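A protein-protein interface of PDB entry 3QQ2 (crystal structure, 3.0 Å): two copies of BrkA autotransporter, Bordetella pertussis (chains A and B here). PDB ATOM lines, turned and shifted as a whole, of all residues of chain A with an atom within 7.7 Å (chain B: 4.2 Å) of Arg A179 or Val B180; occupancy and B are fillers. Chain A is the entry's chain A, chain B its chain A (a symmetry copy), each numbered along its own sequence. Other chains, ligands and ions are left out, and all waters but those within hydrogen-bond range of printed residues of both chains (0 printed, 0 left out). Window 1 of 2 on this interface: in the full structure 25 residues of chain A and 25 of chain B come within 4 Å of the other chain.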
ATOM      1  N   ILE A 121      18.830  35.844 -20.976  1.00  0.00           N
ATOM      2  CA  ILE A 121      18.843  36.638 -19.749  1.00  0.00           C
ATOM      3  C   ILE A 121      19.658  37.922 -19.876  1.00  0.00           C
ATOM      4  O   ILE A 121      20.239  38.202 -20.922  1.00  0.00           O
ATOM      5  CB  ILE A 121      19.336  35.808 -18.530  1.00  0.00           C
ATOM      6  CG1 ILE A 121      18.664  34.429 -18.486  1.00  0.00           C
ATOM      7  CG2 ILE A 121      19.085  36.546 -17.212  1.00  0.00           C
ATOM      8  CD1 ILE A 121      17.141  34.460 -18.368  1.00  0.00           C
ATOM      9  N   VAL A 129      23.608  36.614 -21.125  1.00  0.00           N
ATOM     10  CA  VAL A 129      23.850  35.205 -21.379  1.00  0.00           C
ATOM     11  C   VAL A 129      22.707  34.618 -22.214  1.00  0.00           C
ATOM     12  O   VAL A 129      21.541  34.849 -21.915  1.00  0.00           O
ATOM     13  CB  VAL A 129      24.021  34.437 -20.051  1.00  0.00           C
ATOM     14  CG1 VAL A 129      22.687  34.287 -19.319  1.00  0.00           C
ATOM     15  CG2 VAL A 129      24.646  33.084 -20.278  1.00  0.00           C
ATOM     16  N   ARG A 171      24.716  20.181 -18.561  1.00  0.00           N
ATOM     17  CA  ARG A 171      25.803  21.003 -18.010  1.00  0.00           C
ATOM     18  C   ARG A 171      27.100  20.795 -18.786  1.00  0.00           C
ATOM     19  O   ARG A 171      27.570  19.662 -18.915  1.00  0.00           O
ATOM     20  CB  ARG A 171      26.026  20.669 -16.531  1.00  0.00           C
ATOM     21  CG  ARG A 171      27.214  21.378 -15.841  1.00  0.00           C
ATOM     22  CD  ARG A 171      27.728  20.507 -14.702  1.00  0.00           C
ATOM     23  NE  ARG A 171      26.670  19.581 -14.282  1.00  0.00           N
ATOM     24  CZ  ARG A 171      26.792  18.636 -13.354  1.00  0.00           C
ATOM     25  NH1 ARG A 171      27.949  18.464 -12.709  1.00  0.00           N
ATOM     26  NH2 ARG A 171      25.744  17.859 -13.076  1.00  0.00           N
ATOM     27  N   TYR A 172      27.671  21.890 -19.290  1.00  0.00           N
ATOM     28  CA  TYR A 172      28.958  21.873 -20.013  1.00  0.00           C
ATOM     29  C   TYR A 172      29.928  22.880 -19.373  1.00  0.00           C
ATOM     30  O   TYR A 172      29.694  23.308 -18.236  1.00  0.00           O
ATOM     31  CB  TYR A 172      28.765  22.111 -21.529  1.00  0.00           C
ATOM     32  CG  TYR A 172      27.409  22.679 -21.936  1.00  0.00           C
ATOM     33  CD1 TYR A 172      27.322  23.824 -22.733  1.00  0.00           C
ATOM     34  CD2 TYR A 172      26.204  22.058 -21.544  1.00  0.00           C
ATOM     35  CE1 TYR A 172      26.074  24.348 -23.117  1.00  0.00           C
ATOM     36  CE2 TYR A 172      24.962  22.581 -21.909  1.00  0.00           C
ATOM     37  CZ  TYR A 172      24.914  23.722 -22.695  1.00  0.00           C
ATOM     38  OH  TYR A 172      23.704  24.234 -23.057  1.00  0.00           O
ATOM     39  N   ARG A 173      31.008  23.246 -20.064  1.00  0.00           N
ATOM     40  CA  ARG A 173      31.940  24.198 -19.481  1.00  0.00           C
ATOM     41  C   ARG A 173      33.125  24.622 -20.356  1.00  0.00           C
ATOM     42  O   ARG A 173      34.028  23.826 -20.652  1.00  0.00           O
ATOM     43  CB  ARG A 173      32.411  23.714 -18.100  1.00  0.00           C
ATOM     44  CG  ARG A 173      33.330  22.499 -18.081  1.00  0.00           C
ATOM     45  CD  ARG A 173      34.759  22.946 -17.772  1.00  0.00           C
ATOM     46  NE  ARG A 173      35.595  21.887 -17.200  1.00  0.00           N
ATOM     47  CZ  ARG A 173      35.606  21.542 -15.912  1.00  0.00           C
ATOM     48  NH1 ARG A 173      34.817  22.157 -15.041  1.00  0.00           N
ATOM     49  NH2 ARG A 173      36.404  20.571 -15.494  1.00  0.00           N
ATOM     50  N   ALA A 174      33.110  25.893 -20.760  1.00  0.00           N
ATOM     51  CA  ALA A 174      34.261  26.524 -21.394  1.00  0.00           C
ATOM     52  C   ALA A 174      35.396  26.497 -20.395  1.00  0.00           C
ATOM     53  O   ALA A 174      35.315  27.097 -19.314  1.00  0.00           O
ATOM     54  CB  ALA A 174      33.946  27.959 -21.808  1.00  0.00           C
ATOM     55  N   SER A 175      36.448  25.777 -20.769  1.00  0.00           N
ATOM     56  CA  SER A 175      37.591  25.572 -19.917  1.00  0.00           C
ATOM     57  C   SER A 175      38.214  26.897 -19.543  1.00  0.00           C
ATOM     58  O   SER A 175      38.023  27.910 -20.217  1.00  0.00           O
ATOM     59  CB  SER A 175      38.606  24.674 -20.602  1.00  0.00           C
ATOM     60  OG  SER A 175      39.309  23.909 -19.645  1.00  0.00           O
ATOM     61  N   ASN A 176      38.956  26.856 -18.444  1.00  0.00           N
ATOM     62  CA  ASN A 176      39.550  28.022 -17.791  1.00  0.00           C
ATOM     63  C   ASN A 176      38.665  29.275 -17.787  1.00  0.00           C
ATOM     64  O   ASN A 176      39.152  30.386 -18.042  1.00  0.00           O
ATOM     65  CB  ASN A 176      40.957  28.314 -18.326  1.00  0.00           C
ATOM     66  CG  ASN A 176      41.867  28.894 -17.257  1.00  0.00           C
ATOM     67  OD1 ASN A 176      41.395  29.258 -16.181  1.00  0.00           O
ATOM     68  ND2 ASN A 176      43.177  28.977 -17.539  1.00  0.00           N
ATOM     69  N   GLY A 177      37.374  29.084 -17.491  1.00  0.00           N
ATOM     70  CA  GLY A 177      36.452  30.198 -17.352  1.00  0.00           C
ATOM     71  C   GLY A 177      35.036  29.873 -16.906  1.00  0.00           C
ATOM     72  O   GLY A 177      34.726  29.881 -15.710  1.00  0.00           O
ATOM     73  N   LEU A 178      34.182  29.579 -17.882  1.00  0.00           N
ATOM     74  CA  LEU A 178      32.736  29.660 -17.710  1.00  0.00           C
ATOM     75  C   LEU A 178      32.039  28.323 -17.479  1.00  0.00           C
ATOM     76  O   LEU A 178      32.372  27.323 -18.107  1.00  0.00           O
ATOM     77  CB  LEU A 178      32.131  30.387 -18.918  1.00  0.00           C
ATOM     78  CG  LEU A 178      30.657  30.251 -19.286  1.00  0.00           C
ATOM     79  CD1 LEU A 178      30.152  31.573 -19.793  1.00  0.00           C
ATOM     80  CD2 LEU A 178      30.464  29.149 -20.327  1.00  0.00           C
ATOM     81  N   ARG A 179      31.043  28.329 -16.597  1.00  0.00           N
ATOM     82  CA  ARG A 179      30.301  27.125 -16.257  1.00  0.00           C
ATOM     83  C   ARG A 179      28.787  27.350 -16.370  1.00  0.00           C
ATOM     84  O   ARG A 179      28.250  28.336 -15.861  1.00  0.00           O
ATOM     85  CB  ARG A 179      30.681  26.652 -14.853  1.00  0.00           C
ATOM     86  CG  ARG A 179      30.463  25.166 -14.621  1.00  0.00           C
ATOM     87  CD  ARG A 179      30.492  24.798 -13.131  1.00  0.00           C
ATOM     88  NE  ARG A 179      31.788  24.931 -12.435  1.00  0.00           N
ATOM     89  CZ  ARG A 179      33.004  24.786 -12.971  1.00  0.00           C
ATOM     90  NH1 ARG A 179      33.165  24.505 -14.259  1.00  0.00           N
ATOM     91  NH2 ARG A 179      34.084  24.922 -12.205  1.00  0.00           N
ATOM     92  N   VAL A 180      28.120  26.423 -17.055  1.00  0.00           N
ATOM     93  CA  VAL A 180      26.676  26.472 -17.283  1.00  0.00           C
ATOM     94  C   VAL A 180      26.026  25.170 -16.846  1.00  0.00           C
ATOM     95  O   VAL A 180      26.385  24.098 -17.325  1.00  0.00           O
ATOM     96  CB  VAL A 180      26.329  26.733 -18.769  1.00  0.00           C
ATOM     97  CG1 VAL A 180      27.121  25.802 -19.702  1.00  0.00           C
ATOM     98  CG2 VAL A 180      24.826  26.594 -19.009  1.00  0.00           C
ATOM     99  N   LYS A 181      25.074  25.270 -15.931  1.00  0.00           N
ATOM    100  CA  LYS A 181      24.335  24.105 -15.495  1.00  0.00           C
ATOM    101  C   LYS A 181      22.823  24.331 -15.641  1.00  0.00           C
ATOM    102  O   LYS A 181      22.289  25.359 -15.229  1.00  0.00           O
ATOM    103  CB  LYS A 181      24.729  23.726 -14.063  1.00  0.00           C
ATOM    104  CG  LYS A 181      23.866  22.640 -13.407  1.00  0.00           C
ATOM    105  CD  LYS A 181      24.168  22.490 -11.911  1.00  0.00           C
ATOM    106  CE  LYS A 181      23.889  23.776 -11.128  1.00  0.00           C
ATOM    107  NZ  LYS A 181      24.944  24.071 -10.082  1.00  0.00           N
ATOM    108  N   VAL A 182      22.153  23.382 -16.280  1.00  0.00           N
ATOM    109  CA  VAL A 182      20.708  23.308 -16.242  1.00  0.00           C
ATOM    110  C   VAL A 182      20.414  22.225 -15.230  1.00  0.00           C
ATOM    111  O   VAL A 182      20.971  21.134 -15.305  1.00  0.00           O
ATOM    112  CB  VAL A 182      20.079  22.873 -17.594  1.00  0.00           C
ATOM    113  CG1 VAL A 182      18.594  23.179 -17.582  1.00  0.00           C
ATOM    114  CG2 VAL A 182      20.751  23.558 -18.780  1.00  0.00           C
ATOM    115  N   ARG B 171      28.071  35.372 -11.530  1.00  0.00           N
ATOM    116  CA  ARG B 171      27.123  34.250 -11.498  1.00  0.00           C
ATOM    117  C   ARG B 171      25.696  34.738 -11.267  1.00  0.00           C
ATOM    118  O   ARG B 171      25.430  35.430 -10.282  1.00  0.00           O
ATOM    119  CB  ARG B 171      27.512  33.255 -10.399  1.00  0.00           C
ATOM    120  CG  ARG B 171      26.542  32.073 -10.171  1.00  0.00           C
ATOM    121  CD  ARG B 171      26.643  31.611  -8.723  1.00  0.00           C
ATOM    122  NE  ARG B 171      27.933  32.034  -8.165  1.00  0.00           N
ATOM    123  CZ  ARG B 171      28.330  31.853  -6.909  1.00  0.00           C
ATOM    124  NH1 ARG B 171      27.536  31.239  -6.028  1.00  0.00           N
ATOM    125  NH2 ARG B 171      29.532  32.296  -6.538  1.00  0.00           N
ATOM    126  N   TYR B 172      24.790  34.371 -12.175  1.00  0.00           N
ATOM    127  CA  TYR B 172      23.356  34.706 -12.070  1.00  0.00           C
ATOM    128  C   TYR B 172      22.513  33.426 -12.177  1.00  0.00           C
ATOM    129  O   TYR B 172      23.056  32.325 -12.012  1.00  0.00           O
ATOM    130  CB  TYR B 172      22.943  35.782 -13.102  1.00  0.00           C
ATOM    131  CG  TYR B 172      23.932  36.010 -14.241  1.00  0.00           C
ATOM    132  CD1 TYR B 172      23.513  35.962 -15.574  1.00  0.00           C
ATOM    133  CD2 TYR B 172      25.290  36.299 -13.988  1.00  0.00           C
ATOM    134  CE1 TYR B 172      24.419  36.180 -16.628  1.00  0.00           C
ATOM    135  CE2 TYR B 172      26.198  36.501 -15.030  1.00  0.00           C
ATOM    136  CZ  TYR B 172      25.748  36.440 -16.340  1.00  0.00           C
ATOM    137  OH  TYR B 172      26.629  36.640 -17.359  1.00  0.00           O
ATOM    138  N   ARG B 179      21.481  27.795 -14.600  1.00  0.00           N
ATOM    139  CA  ARG B 179      22.505  28.387 -13.754  1.00  0.00           C
ATOM    140  C   ARG B 179      23.808  28.621 -14.532  1.00  0.00           C
ATOM    141  O   ARG B 179      24.299  27.734 -15.233  1.00  0.00           O
ATOM    142  CB  ARG B 179      22.750  27.505 -12.528  1.00  0.00           C
ATOM    143  CG  ARG B 179      23.308  28.254 -11.330  1.00  0.00           C
ATOM    144  CD  ARG B 179      23.885  27.307 -10.268  1.00  0.00           C
ATOM    145  NE  ARG B 179      22.925  26.445  -9.550  1.00  0.00           N
ATOM    146  CZ  ARG B 179      21.647  26.725  -9.274  1.00  0.00           C
ATOM    147  NH1 ARG B 179      21.089  27.867  -9.657  1.00  0.00           N
ATOM    148  NH2 ARG B 179      20.910  25.846  -8.599  1.00  0.00           N
ATOM    149  N   VAL B 180      24.344  29.833 -14.400  1.00  0.00           N
ATOM    150  CA  VAL B 180      25.573  30.249 -15.074  1.00  0.00           C
ATOM    151  C   VAL B 180      26.565  30.808 -14.069  1.00  0.00           C
ATOM    152  O   VAL B 180      26.264  31.757 -13.350  1.00  0.00           O
ATOM    153  CB  VAL B 180      25.307  31.316 -16.165  1.00  0.00           C
ATOM    154  CG1 VAL B 180      24.420  32.454 -15.633  1.00  0.00           C
ATOM    155  CG2 VAL B 180      26.622  31.865 -16.720  1.00  0.00           C
ATOM    156  N   LYS B 181      27.747  30.211 -14.020  1.00  0.00           N
ATOM    157  CA  LYS B 181      28.794  30.705 -13.154  1.00  0.00           C
ATOM    158  C   LYS B 181      30.083  30.964 -13.949  1.00  0.00           C
ATOM    159  O   LYS B 181      30.529  30.126 -14.730  1.00  0.00           O
ATOM    160  CB  LYS B 181      29.019  29.743 -11.982  1.00  0.00           C
ATOM    161  CG  LYS B 181      30.246  30.040 -11.109  1.00  0.00           C
ATOM    162  CD  LYS B 181      30.535  28.908 -10.116  1.00  0.00           C
ATOM    163  CE  LYS B 181      30.834  27.580 -10.817  1.00  0.00           C
ATOM    164  NZ  LYS B 181      30.190  26.393 -10.132  1.00  0.00           N
ATOM    165  N   ASP B 183      33.916  31.609 -13.018  1.00  0.00           N
ATOM    166  CA  ASP B 183      34.709  31.434 -11.830  1.00  0.00           C
ATOM    167  C   ASP B 183      35.795  32.474 -11.689  1.00  0.00           C
ATOM    168  O   ASP B 183      36.532  32.748 -12.637  1.00  0.00           O
ATOM    169  CB  ASP B 183      35.304  30.038 -11.797  1.00  0.00           C
ATOM    170  CG  ASP B 183      34.531  29.113 -10.908  1.00  0.00           C
ATOM    171  OD1 ASP B 183      34.752  27.892 -11.014  1.00  0.00           O
ATOM    172  OD2 ASP B 183      33.704  29.596 -10.099  1.00  0.00           O
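The backbone NH (N) of Asp B183 is in hydrogen-bond range of the backbone carbonyl oxygen (O) of Gly A177 (3.3 Å). The backbone carbonyl oxygen (O) of Lys B181 lies within hydrogen-bond range of the backbone NH (N) of Arg A179, 2.6 Å away. The guanidinium group of Arg A179 is in salt-bridge range of the side-chain carboxylate of Asp B183, at 3.3 Å. The backbone carbonyl oxygen of Lys A181 sits at hydrogen-bond distance from the backbone NH of Arg B179, at 2.6 Å.
N of Ile A121 is in hydrogen-bond range of O of Val A129, at 3.0 Å. The backbone NH (N) of Tyr A172 lies within hydrogen-bond range of the backbone carbonyl oxygen (O) of Val A180. The backbone NH (N) of Tyr B172 lies within hydrogen-bond range of the backbone carbonyl oxygen (O) of Val B180 (3.2 Å).
CG1 of Val A129 touches CE1 of Tyr B172, at 3.7 Å. Lys B181 touches Leu A178 (O to C, 3.6 Å). Arg A179 touches Val B180. Val A180 touches Arg B179 (CA to O, 3.4 Å).
Arg A179 touches three residues of chain B. Of the printed residues of chain A, Lys B181 touches Leu A178 and Arg A179. Printed residues of chain A within 4 Å of Arg B179: Val A180 and Lys A181. Printed residues of chain B within 4 Å of Val A180: Arg B179. Of the printed residues of chain B, Lys A181 touches Arg B179. Of the printed residues of chain B, Gly A177 touches Asp B183 (3.3 Å). Arg A173 touches none of the printed residues of chain B. Ile A121 touches none of the printed residues of chain B. The nearest residue of chain A that does not touch Val B180 is Val A129 (4.2 Å). The nearest printed residue of chain B that does not touch Gly A177 is Lys B181 (4.3 Å).
Printed residues of chain B that touch a printed residue of chain A: Tyr B172, Arg B179, Val B180, Lys B181 and Asp B183. Hydrophobic or aromatic side chains of chain B that line the printed part of chain A: Tyr B172 and Val B180. Of the 14 printed residues of chain A, 6 touch a printed residue of chain B. Printed residues of chain A that touch a printed residue of chain B: Val A129, Gly A177, Leu A178, Arg A179, Val A180 and Lys A181. Hydrophobic or aromatic side chains of chain A within 4 Å of the printed part of chain B: Val A129 and Val A180. Among the printed residues, Asp or Glu carboxylates within 4 Å of a Lys or Arg side-chain nitrogen of the other chain: Arg A179 with Asp B183 (3.3 Å).
Arg A179 touches Val B180, and with the chains exchanged Val A180 touches Arg B179. Arg A179 touches Lys B181, and with the chains exchanged Lys A181 touches Arg B179. Of the 8 pairs that touch across the chains among the printed residues, 4 have their exchanged pair printed and touching as well.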
